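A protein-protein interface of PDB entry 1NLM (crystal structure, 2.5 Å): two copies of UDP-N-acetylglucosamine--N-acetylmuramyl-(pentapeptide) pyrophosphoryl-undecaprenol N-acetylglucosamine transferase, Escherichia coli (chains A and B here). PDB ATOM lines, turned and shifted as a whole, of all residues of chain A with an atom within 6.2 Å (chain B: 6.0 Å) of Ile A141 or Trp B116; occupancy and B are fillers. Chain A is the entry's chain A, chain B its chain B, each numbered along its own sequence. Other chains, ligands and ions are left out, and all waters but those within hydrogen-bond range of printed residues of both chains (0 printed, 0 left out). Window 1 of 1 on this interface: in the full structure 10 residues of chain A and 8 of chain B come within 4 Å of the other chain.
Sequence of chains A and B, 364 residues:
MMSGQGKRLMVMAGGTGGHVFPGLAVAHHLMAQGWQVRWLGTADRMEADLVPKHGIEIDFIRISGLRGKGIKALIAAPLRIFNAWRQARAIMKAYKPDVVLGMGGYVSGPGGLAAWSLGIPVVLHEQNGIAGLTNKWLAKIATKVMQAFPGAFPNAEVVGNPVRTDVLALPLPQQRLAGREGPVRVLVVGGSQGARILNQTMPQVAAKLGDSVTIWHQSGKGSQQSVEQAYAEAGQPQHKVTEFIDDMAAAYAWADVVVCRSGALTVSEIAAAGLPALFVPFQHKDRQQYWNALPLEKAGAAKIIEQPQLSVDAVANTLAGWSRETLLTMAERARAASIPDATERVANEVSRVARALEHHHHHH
Lys B140 touches its own counterpart, Lys A140.
Ile A141 touches Trp B116, but with the chains exchanged Trp A116 does not touch Ile B141 (4.2 Å).
Ile A141 touches Lys B140, but with the chains exchanged Lys A140 does not touch Ile B141 (5.7 Å).
Ala A142 touches Lys B140, but with the chains exchanged Lys A140 does not touch Ala B142 (7.4 Å).
8 positions are printed for both chains.
Of the printed residues of chain B, Lys A140 touches Trp B116 (3.9 Å) and Lys B140 (3.9 Å).
Of chain B, only Trp B116 (3.5 Å) and Lys B140 (3.4 Å) come within 4 Å of Ile A141.
Of the printed residues of chain A, Trp B116 touches Lys A140 (3.9 Å) and Ile A141 (3.5 Å).
Of the printed residues of chain A, Ser B117 touches Ile A75 (3.5 Å).
Of the printed residues of chain A, Lys B140 touches Trp A116 (3.8 Å), Lys A140 (3.9 Å), Ile A141 (3.4 Å) and Ala A142 (3.4 Å).
The nearest printed residue of chain B that does not touch Lys A140 is Ile B141 (5.7 Å).
Hydrophobic or aromatic side chains of chain B that line the printed part of chain A: Trp B116.
Among the printed residues, no Asp or Glu carboxylate lies within 4 Å of a Lys or Arg side-chain nitrogen of the other chain.
The backbone carbonyl oxygen (O) of Ile A141 lies close to the side-chain amino group (NZ) of Lys B140 (3.5 Å).
The side-chain amino group of Lys B140 is in hydrogen-bond range of the backbone carbonyl oxygen of Ala A142, 3.4 Å away.
O of Leu B113 sits at hydrogen-bond distance from OG of Ser B117 (3.2 Å).
The backbone carbonyl oxygen of Ala B114 sits at hydrogen-bond distance from the side-chain hydroxyl of Ser B117 (2.7 Å).
Among the printed residues, merely in contact across the chains: Ile A75 with Ser B117, Trp A116 with Lys B140, Lys A140 with Trp B116, Lys A140 with Lys B140 and Ile A141 with Trp B116.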
ATOM      1  N   ILE A  75     -19.966  -0.684  -1.643  1.00  0.00           N
ATOM      2  CA  ILE A  75     -20.078  -1.777  -0.677  1.00  0.00           C
ATOM      3  C   ILE A  75     -20.042  -3.065  -1.485  1.00  0.00           C
ATOM      4  O   ILE A  75     -19.362  -4.021  -1.118  1.00  0.00           O
ATOM      5  CB  ILE A  75     -21.420  -1.730   0.132  1.00  0.00           C
ATOM      6  CG1 ILE A  75     -21.265  -0.853   1.385  1.00  0.00           C
ATOM      7  CG2 ILE A  75     -21.803  -3.121   0.594  1.00  0.00           C
ATOM      8  CD1 ILE A  75     -20.735   0.548   1.131  1.00  0.00           C
ATOM      9  N   GLY A 109     -13.711  11.012  -2.582  1.00  0.00           N
ATOM     10  CA  GLY A 109     -13.719   9.707  -1.926  1.00  0.00           C
ATOM     11  C   GLY A 109     -12.320   9.151  -1.700  1.00  0.00           C
ATOM     12  O   GLY A 109     -11.918   8.911  -0.565  1.00  0.00           O
ATOM     13  N   GLY A 112     -10.132  11.356   0.570  1.00  0.00           N
ATOM     14  CA  GLY A 112     -10.523  11.308   1.967  1.00  0.00           C
ATOM     15  C   GLY A 112     -10.035  10.027   2.621  1.00  0.00           C
ATOM     16  O   GLY A 112      -9.418  10.060   3.686  1.00  0.00           O
ATOM     17  N   LEU A 113     -10.313   8.894   1.984  1.00  0.00           N
ATOM     18  CA  LEU A 113      -9.877   7.612   2.507  1.00  0.00           C
ATOM     19  C   LEU A 113      -8.364   7.615   2.676  1.00  0.00           C
ATOM     20  O   LEU A 113      -7.842   7.094   3.654  1.00  0.00           O
ATOM     21  CB  LEU A 113     -10.273   6.490   1.554  1.00  0.00           C
ATOM     22  CG  LEU A 113     -11.751   6.130   1.510  1.00  0.00           C
ATOM     23  CD1 LEU A 113     -11.976   5.097   0.416  1.00  0.00           C
ATOM     24  CD2 LEU A 113     -12.189   5.594   2.862  1.00  0.00           C
ATOM     25  N   ALA A 114      -7.670   8.203   1.707  1.00  0.00           N
ATOM     26  CA  ALA A 114      -6.217   8.278   1.731  1.00  0.00           C
ATOM     27  C   ALA A 114      -5.719   9.124   2.901  1.00  0.00           C
ATOM     28  O   ALA A 114      -4.838   8.706   3.646  1.00  0.00           O
ATOM     29  CB  ALA A 114      -5.725   8.856   0.428  1.00  0.00           C
ATOM     30  N   TRP A 116      -7.188   9.800   5.633  1.00  0.00           N
ATOM     31  CA  TRP A 116      -7.533   9.053   6.832  1.00  0.00           C
ATOM     32  C   TRP A 116      -6.631   7.843   7.092  1.00  0.00           C
ATOM     33  O   TRP A 116      -6.325   7.538   8.247  1.00  0.00           O
ATOM     34  CB  TRP A 116      -8.989   8.605   6.730  1.00  0.00           C
ATOM     35  CG  TRP A 116      -9.458   7.736   7.843  1.00  0.00           C
ATOM     36  CD1 TRP A 116      -9.615   8.082   9.157  1.00  0.00           C
ATOM     37  CD2 TRP A 116      -9.885   6.374   7.730  1.00  0.00           C
ATOM     38  NE1 TRP A 116     -10.120   7.018   9.871  1.00  0.00           N
ATOM     39  CE2 TRP A 116     -10.296   5.957   9.018  1.00  0.00           C
ATOM     40  CE3 TRP A 116      -9.967   5.467   6.665  1.00  0.00           C
ATOM     41  CZ2 TRP A 116     -10.782   4.669   9.267  1.00  0.00           C
ATOM     42  CZ3 TRP A 116     -10.451   4.187   6.913  1.00  0.00           C
ATOM     43  CH2 TRP A 116     -10.852   3.801   8.205  1.00  0.00           C
ATOM     44  N   VAL A 122      -9.156  14.990   8.117  1.00  0.00           N
ATOM     45  CA  VAL A 122      -9.954  15.326   6.946  1.00  0.00           C
ATOM     46  C   VAL A 122     -11.171  16.175   7.339  1.00  0.00           C
ATOM     47  O   VAL A 122     -11.952  15.808   8.213  1.00  0.00           O
ATOM     48  CB  VAL A 122     -10.376  14.038   6.187  1.00  0.00           C
ATOM     49  CG1 VAL A 122     -10.483  12.888   7.160  1.00  0.00           C
ATOM     50  CG2 VAL A 122     -11.697  14.248   5.475  1.00  0.00           C
ATOM     51  N   TRP A 137     -20.900   9.146   2.650  1.00  0.00           N
ATOM     52  CA  TRP A 137     -20.106   8.061   3.224  1.00  0.00           C
ATOM     53  C   TRP A 137     -18.716   8.470   3.688  1.00  0.00           C
ATOM     54  O   TRP A 137     -18.087   7.765   4.472  1.00  0.00           O
ATOM     55  CB  TRP A 137     -19.968   6.907   2.233  1.00  0.00           C
ATOM     56  CG  TRP A 137     -19.062   7.175   1.061  1.00  0.00           C
ATOM     57  CD1 TRP A 137     -19.445   7.479  -0.213  1.00  0.00           C
ATOM     58  CD2 TRP A 137     -17.627   7.072   1.034  1.00  0.00           C
ATOM     59  NE1 TRP A 137     -18.346   7.559  -1.034  1.00  0.00           N
ATOM     60  CE2 TRP A 137     -17.217   7.315  -0.296  1.00  0.00           C
ATOM     61  CE3 TRP A 137     -16.651   6.795   2.003  1.00  0.00           C
ATOM     62  CZ2 TRP A 137     -15.868   7.285  -0.687  1.00  0.00           C
ATOM     63  CZ3 TRP A 137     -15.310   6.765   1.616  1.00  0.00           C
ATOM     64  CH2 TRP A 137     -14.934   7.008   0.281  1.00  0.00           C
ATOM     65  N   LEU A 138     -18.240   9.607   3.196  1.00  0.00           N
ATOM     66  CA  LEU A 138     -16.919  10.101   3.556  1.00  0.00           C
ATOM     67  C   LEU A 138     -16.959  10.777   4.920  1.00  0.00           C
ATOM     68  O   LEU A 138     -15.931  10.944   5.568  1.00  0.00           O
ATOM     69  CB  LEU A 138     -16.439  11.082   2.490  1.00  0.00           C
ATOM     70  CG  LEU A 138     -14.975  11.503   2.456  1.00  0.00           C
ATOM     71  CD1 LEU A 138     -14.071  10.292   2.313  1.00  0.00           C
ATOM     72  CD2 LEU A 138     -14.782  12.455   1.281  1.00  0.00           C
ATOM     73  N   ALA A 139     -18.154  11.159   5.351  1.00  0.00           N
ATOM     74  CA  ALA A 139     -18.327  11.817   6.639  1.00  0.00           C
ATOM     75  C   ALA A 139     -17.894  10.883   7.753  1.00  0.00           C
ATOM     76  O   ALA A 139     -17.323  11.313   8.750  1.00  0.00           O
ATOM     77  CB  ALA A 139     -19.782  12.212   6.831  1.00  0.00           C
ATOM     78  N   LYS A 140     -18.169   9.597   7.567  1.00  0.00           N
ATOM     79  CA  LYS A 140     -17.831   8.577   8.547  1.00  0.00           C
ATOM     80  C   LYS A 140     -16.391   8.681   9.048  1.00  0.00           C
ATOM     81  O   LYS A 140     -16.131   8.537  10.241  1.00  0.00           O
ATOM     82  CB  LYS A 140     -18.075   7.192   7.949  1.00  0.00           C
ATOM     83  CG  LYS A 140     -19.500   6.988   7.450  1.00  0.00           C
ATOM     84  CD  LYS A 140     -20.511   7.150   8.579  1.00  0.00           C
ATOM     85  CE  LYS A 140     -21.948   7.043   8.080  1.00  0.00           C
ATOM     86  NZ  LYS A 140     -22.323   8.173   7.183  1.00  0.00           N
ATOM     87  N   ILE A 141     -15.457   8.947   8.142  1.00  0.00           N
ATOM     88  CA  ILE A 141     -14.051   9.051   8.522  1.00  0.00           C
ATOM     89  C   ILE A 141     -13.536  10.485   8.605  1.00  0.00           C
ATOM     90  O   ILE A 141     -12.337  10.722   8.514  1.00  0.00           O
ATOM     91  CB  ILE A 141     -13.162   8.275   7.532  1.00  0.00           C
ATOM     92  CG1 ILE A 141     -13.422   8.763   6.109  1.00  0.00           C
ATOM     93  CG2 ILE A 141     -13.451   6.797   7.629  1.00  0.00           C
ATOM     94  CD1 ILE A 141     -12.525   8.133   5.085  1.00  0.00           C
ATOM     95  N   ALA A 142     -14.440  11.437   8.793  1.00  0.00           N
ATOM     96  CA  ALA A 142     -14.049  12.841   8.859  1.00  0.00           C
ATOM     97  C   ALA A 142     -13.761  13.338  10.267  1.00  0.00           C
ATOM     98  O   ALA A 142     -14.352  12.873  11.233  1.00  0.00           O
ATOM     99  CB  ALA A 142     -15.126  13.700   8.233  1.00  0.00           C
ATOM    100  N   THR A 143     -12.848  14.297  10.376  1.00  0.00           N
ATOM    101  CA  THR A 143     -12.526  14.863  11.674  1.00  0.00           C
ATOM    102  C   THR A 143     -13.512  15.991  11.992  1.00  0.00           C
ATOM    103  O   THR A 143     -13.914  16.168  13.143  1.00  0.00           O
ATOM    104  CB  THR A 143     -11.086  15.396  11.704  1.00  0.00           C
ATOM    105  OG1 THR A 143     -10.173  14.288  11.680  1.00  0.00           O
ATOM    106  CG2 THR A 143     -10.846  16.226  12.955  1.00  0.00           C
ATOM    107  N   GLY B 111     -12.230  -7.947  11.183  1.00  0.00           N
ATOM    108  CA  GLY B 111     -13.665  -8.177  11.134  1.00  0.00           C
ATOM    109  C   GLY B 111     -14.487  -6.906  11.227  1.00  0.00           C
ATOM    110  O   GLY B 111     -15.574  -6.818  10.647  1.00  0.00           O
ATOM    111  N   GLY B 112     -13.973  -5.923  11.965  1.00  0.00           N
ATOM    112  CA  GLY B 112     -14.668  -4.657  12.109  1.00  0.00           C
ATOM    113  C   GLY B 112     -14.623  -3.891  10.797  1.00  0.00           C
ATOM    114  O   GLY B 112     -15.640  -3.380  10.320  1.00  0.00           O
ATOM    115  N   LEU B 113     -13.431  -3.810  10.215  1.00  0.00           N
ATOM    116  CA  LEU B 113     -13.258  -3.127   8.948  1.00  0.00           C
ATOM    117  C   LEU B 113     -14.148  -3.802   7.914  1.00  0.00           C
ATOM    118  O   LEU B 113     -14.770  -3.136   7.090  1.00  0.00           O
ATOM    119  CB  LEU B 113     -11.798  -3.197   8.497  1.00  0.00           C
ATOM    120  CG  LEU B 113     -10.798  -2.412   9.344  1.00  0.00           C
ATOM    121  CD1 LEU B 113      -9.389  -2.722   8.874  1.00  0.00           C
ATOM    122  CD2 LEU B 113     -11.084  -0.926   9.240  1.00  0.00           C
ATOM    123  N   ALA B 114     -14.208  -5.128   7.968  1.00  0.00           N
ATOM    124  CA  ALA B 114     -15.027  -5.891   7.034  1.00  0.00           C
ATOM    125  C   ALA B 114     -16.503  -5.569   7.219  1.00  0.00           C
ATOM    126  O   ALA B 114     -17.197  -5.227   6.261  1.00  0.00           O
ATOM    127  CB  ALA B 114     -14.797  -7.375   7.233  1.00  0.00           C
ATOM    128  N   ALA B 115     -16.980  -5.688   8.455  1.00  0.00           N
ATOM    129  CA  ALA B 115     -18.377  -5.407   8.764  1.00  0.00           C
ATOM    130  C   ALA B 115     -18.728  -3.964   8.411  1.00  0.00           C
ATOM    131  O   ALA B 115     -19.861  -3.667   8.023  1.00  0.00           O
ATOM    132  CB  ALA B 115     -18.641  -5.660  10.241  1.00  0.00           C
ATOM    133  N   TRP B 116     -17.749  -3.072   8.536  1.00  0.00           N
ATOM    134  CA  TRP B 116     -17.953  -1.659   8.242  1.00  0.00           C
ATOM    135  C   TRP B 116     -18.028  -1.423   6.745  1.00  0.00           C
ATOM    136  O   TRP B 116     -18.837  -0.624   6.279  1.00  0.00           O
ATOM    137  CB  TRP B 116     -16.811  -0.827   8.825  1.00  0.00           C
ATOM    138  CG  TRP B 116     -16.973   0.660   8.644  1.00  0.00           C
ATOM    139  CD1 TRP B 116     -17.957   1.453   9.170  1.00  0.00           C
ATOM    140  CD2 TRP B 116     -16.092   1.537   7.936  1.00  0.00           C
ATOM    141  NE1 TRP B 116     -17.737   2.768   8.839  1.00  0.00           N
ATOM    142  CE2 TRP B 116     -16.600   2.849   8.081  1.00  0.00           C
ATOM    143  CE3 TRP B 116     -14.919   1.343   7.193  1.00  0.00           C
ATOM    144  CZ2 TRP B 116     -15.973   3.961   7.513  1.00  0.00           C
ATOM    145  CZ3 TRP B 116     -14.295   2.451   6.627  1.00  0.00           C
ATOM    146  CH2 TRP B 116     -14.826   3.744   6.792  1.00  0.00           C
ATOM    147  N   SER B 117     -17.171  -2.118   6.004  1.00  0.00           N
ATOM    148  CA  SER B 117     -17.123  -2.000   4.553  1.00  0.00           C
ATOM    149  C   SER B 117     -18.326  -2.672   3.930  1.00  0.00           C
ATOM    150  O   SER B 117     -18.542  -2.575   2.721  1.00  0.00           O
ATOM    151  CB  SER B 117     -15.846  -2.644   4.001  1.00  0.00           C
ATOM    152  OG  SER B 117     -15.820  -4.037   4.245  1.00  0.00           O
ATOM    153  N   LEU B 118     -19.095  -3.371   4.758  1.00  0.00           N
ATOM    154  CA  LEU B 118     -20.291  -4.056   4.295  1.00  0.00           C
ATOM    155  C   LEU B 118     -21.514  -3.358   4.864  1.00  0.00           C
ATOM    156  O   LEU B 118     -22.634  -3.862   4.763  1.00  0.00           O
ATOM    157  CB  LEU B 118     -20.279  -5.522   4.731  1.00  0.00           C
ATOM    158  CG  LEU B 118     -19.261  -6.406   4.001  1.00  0.00           C
ATOM    159  CD1 LEU B 118     -19.241  -7.800   4.611  1.00  0.00           C
ATOM    160  CD2 LEU B 118     -19.624  -6.476   2.518  1.00  0.00           C
ATOM    161  N   GLY B 119     -21.287  -2.195   5.468  1.00  0.00           N
ATOM    162  CA  GLY B 119     -22.379  -1.435   6.045  1.00  0.00           C
ATOM    163  C   GLY B 119     -23.006  -2.094   7.258  1.00  0.00           C
ATOM    164  O   GLY B 119     -24.027  -1.624   7.764  1.00  0.00           O
ATOM    165  N   ILE B 120     -22.407  -3.185   7.733  1.00  0.00           N
ATOM    166  CA  ILE B 120     -22.931  -3.884   8.901  1.00  0.00           C
ATOM    167  C   ILE B 120     -22.570  -3.093  10.157  1.00  0.00           C
ATOM    168  O   ILE B 120     -21.413  -2.717  10.360  1.00  0.00           O
ATOM    169  CB  ILE B 120     -22.349  -5.309   9.021  1.00  0.00           C
ATOM    170  CG1 ILE B 120     -22.632  -6.106   7.747  1.00  0.00           C
ATOM    171  CG2 ILE B 120     -22.960  -6.014  10.220  1.00  0.00           C
ATOM    172  CD1 ILE B 120     -21.969  -7.487   7.720  1.00  0.00           C
ATOM    173  N   VAL B 122     -21.456  -1.925  13.790  1.00  0.00           N
ATOM    174  CA  VAL B 122     -20.387  -2.416  14.628  1.00  0.00           C
ATOM    175  C   VAL B 122     -20.659  -1.967  16.064  1.00  0.00           C
ATOM    176  O   VAL B 122     -20.966  -0.792  16.314  1.00  0.00           O
ATOM    177  CB  VAL B 122     -19.027  -1.855  14.143  1.00  0.00           C
ATOM    178  CG1 VAL B 122     -17.914  -2.253  15.108  1.00  0.00           C
ATOM    179  CG2 VAL B 122     -18.729  -2.368  12.745  1.00  0.00           C
ATOM    180  N   LYS B 140     -13.641   4.262  15.586  1.00  0.00           N
ATOM    181  CA  LYS B 140     -14.003   5.410  14.765  1.00  0.00           C
ATOM    182  C   LYS B 140     -15.062   5.014  13.745  1.00  0.00           C
ATOM    183  O   LYS B 140     -15.810   5.857  13.256  1.00  0.00           O
ATOM    184  CB  LYS B 140     -12.770   5.984  14.058  1.00  0.00           C
ATOM    185  CG  LYS B 140     -12.946   7.436  13.618  1.00  0.00           C
ATOM    186  CD  LYS B 140     -11.634   8.057  13.152  1.00  0.00           C
ATOM    187  CE  LYS B 140     -11.776   9.557  12.914  1.00  0.00           C
ATOM    188  NZ  LYS B 140     -12.790   9.873  11.865  1.00  0.00           N
ATOM    189  N   ILE B 141     -15.128   3.723  13.432  1.00  0.00           N
ATOM    190  CA  ILE B 141     -16.113   3.226  12.483  1.00  0.00           C
ATOM    191  C   ILE B 141     -17.146   2.383  13.212  1.00  0.00           C
ATOM    192  O   ILE B 141     -17.770   1.505  12.619  1.00  0.00           O
ATOM    193  CB  ILE B 141     -15.469   2.353  11.388  1.00  0.00           C
ATOM    194  CG1 ILE B 141     -14.873   1.086  12.001  1.00  0.00           C
ATOM    195  CG2 ILE B 141     -14.395   3.143  10.660  1.00  0.00           C
ATOM    196  CD1 ILE B 141     -14.329   0.108  10.969  1.00  0.00           C
ATOM    197  N   ALA B 142     -17.323   2.647  14.501  1.00  0.00           N
ATOM    198  CA  ALA B 142     -18.283   1.894  15.300  1.00  0.00           C
ATOM    199  C   ALA B 142     -19.593   2.657  15.425  1.00  0.00           C
ATOM    200  O   ALA B 142     -19.601   3.884  15.472  1.00  0.00           O
ATOM    201  CB  ALA B 142     -17.712   1.612  16.692  1.00  0.00           C
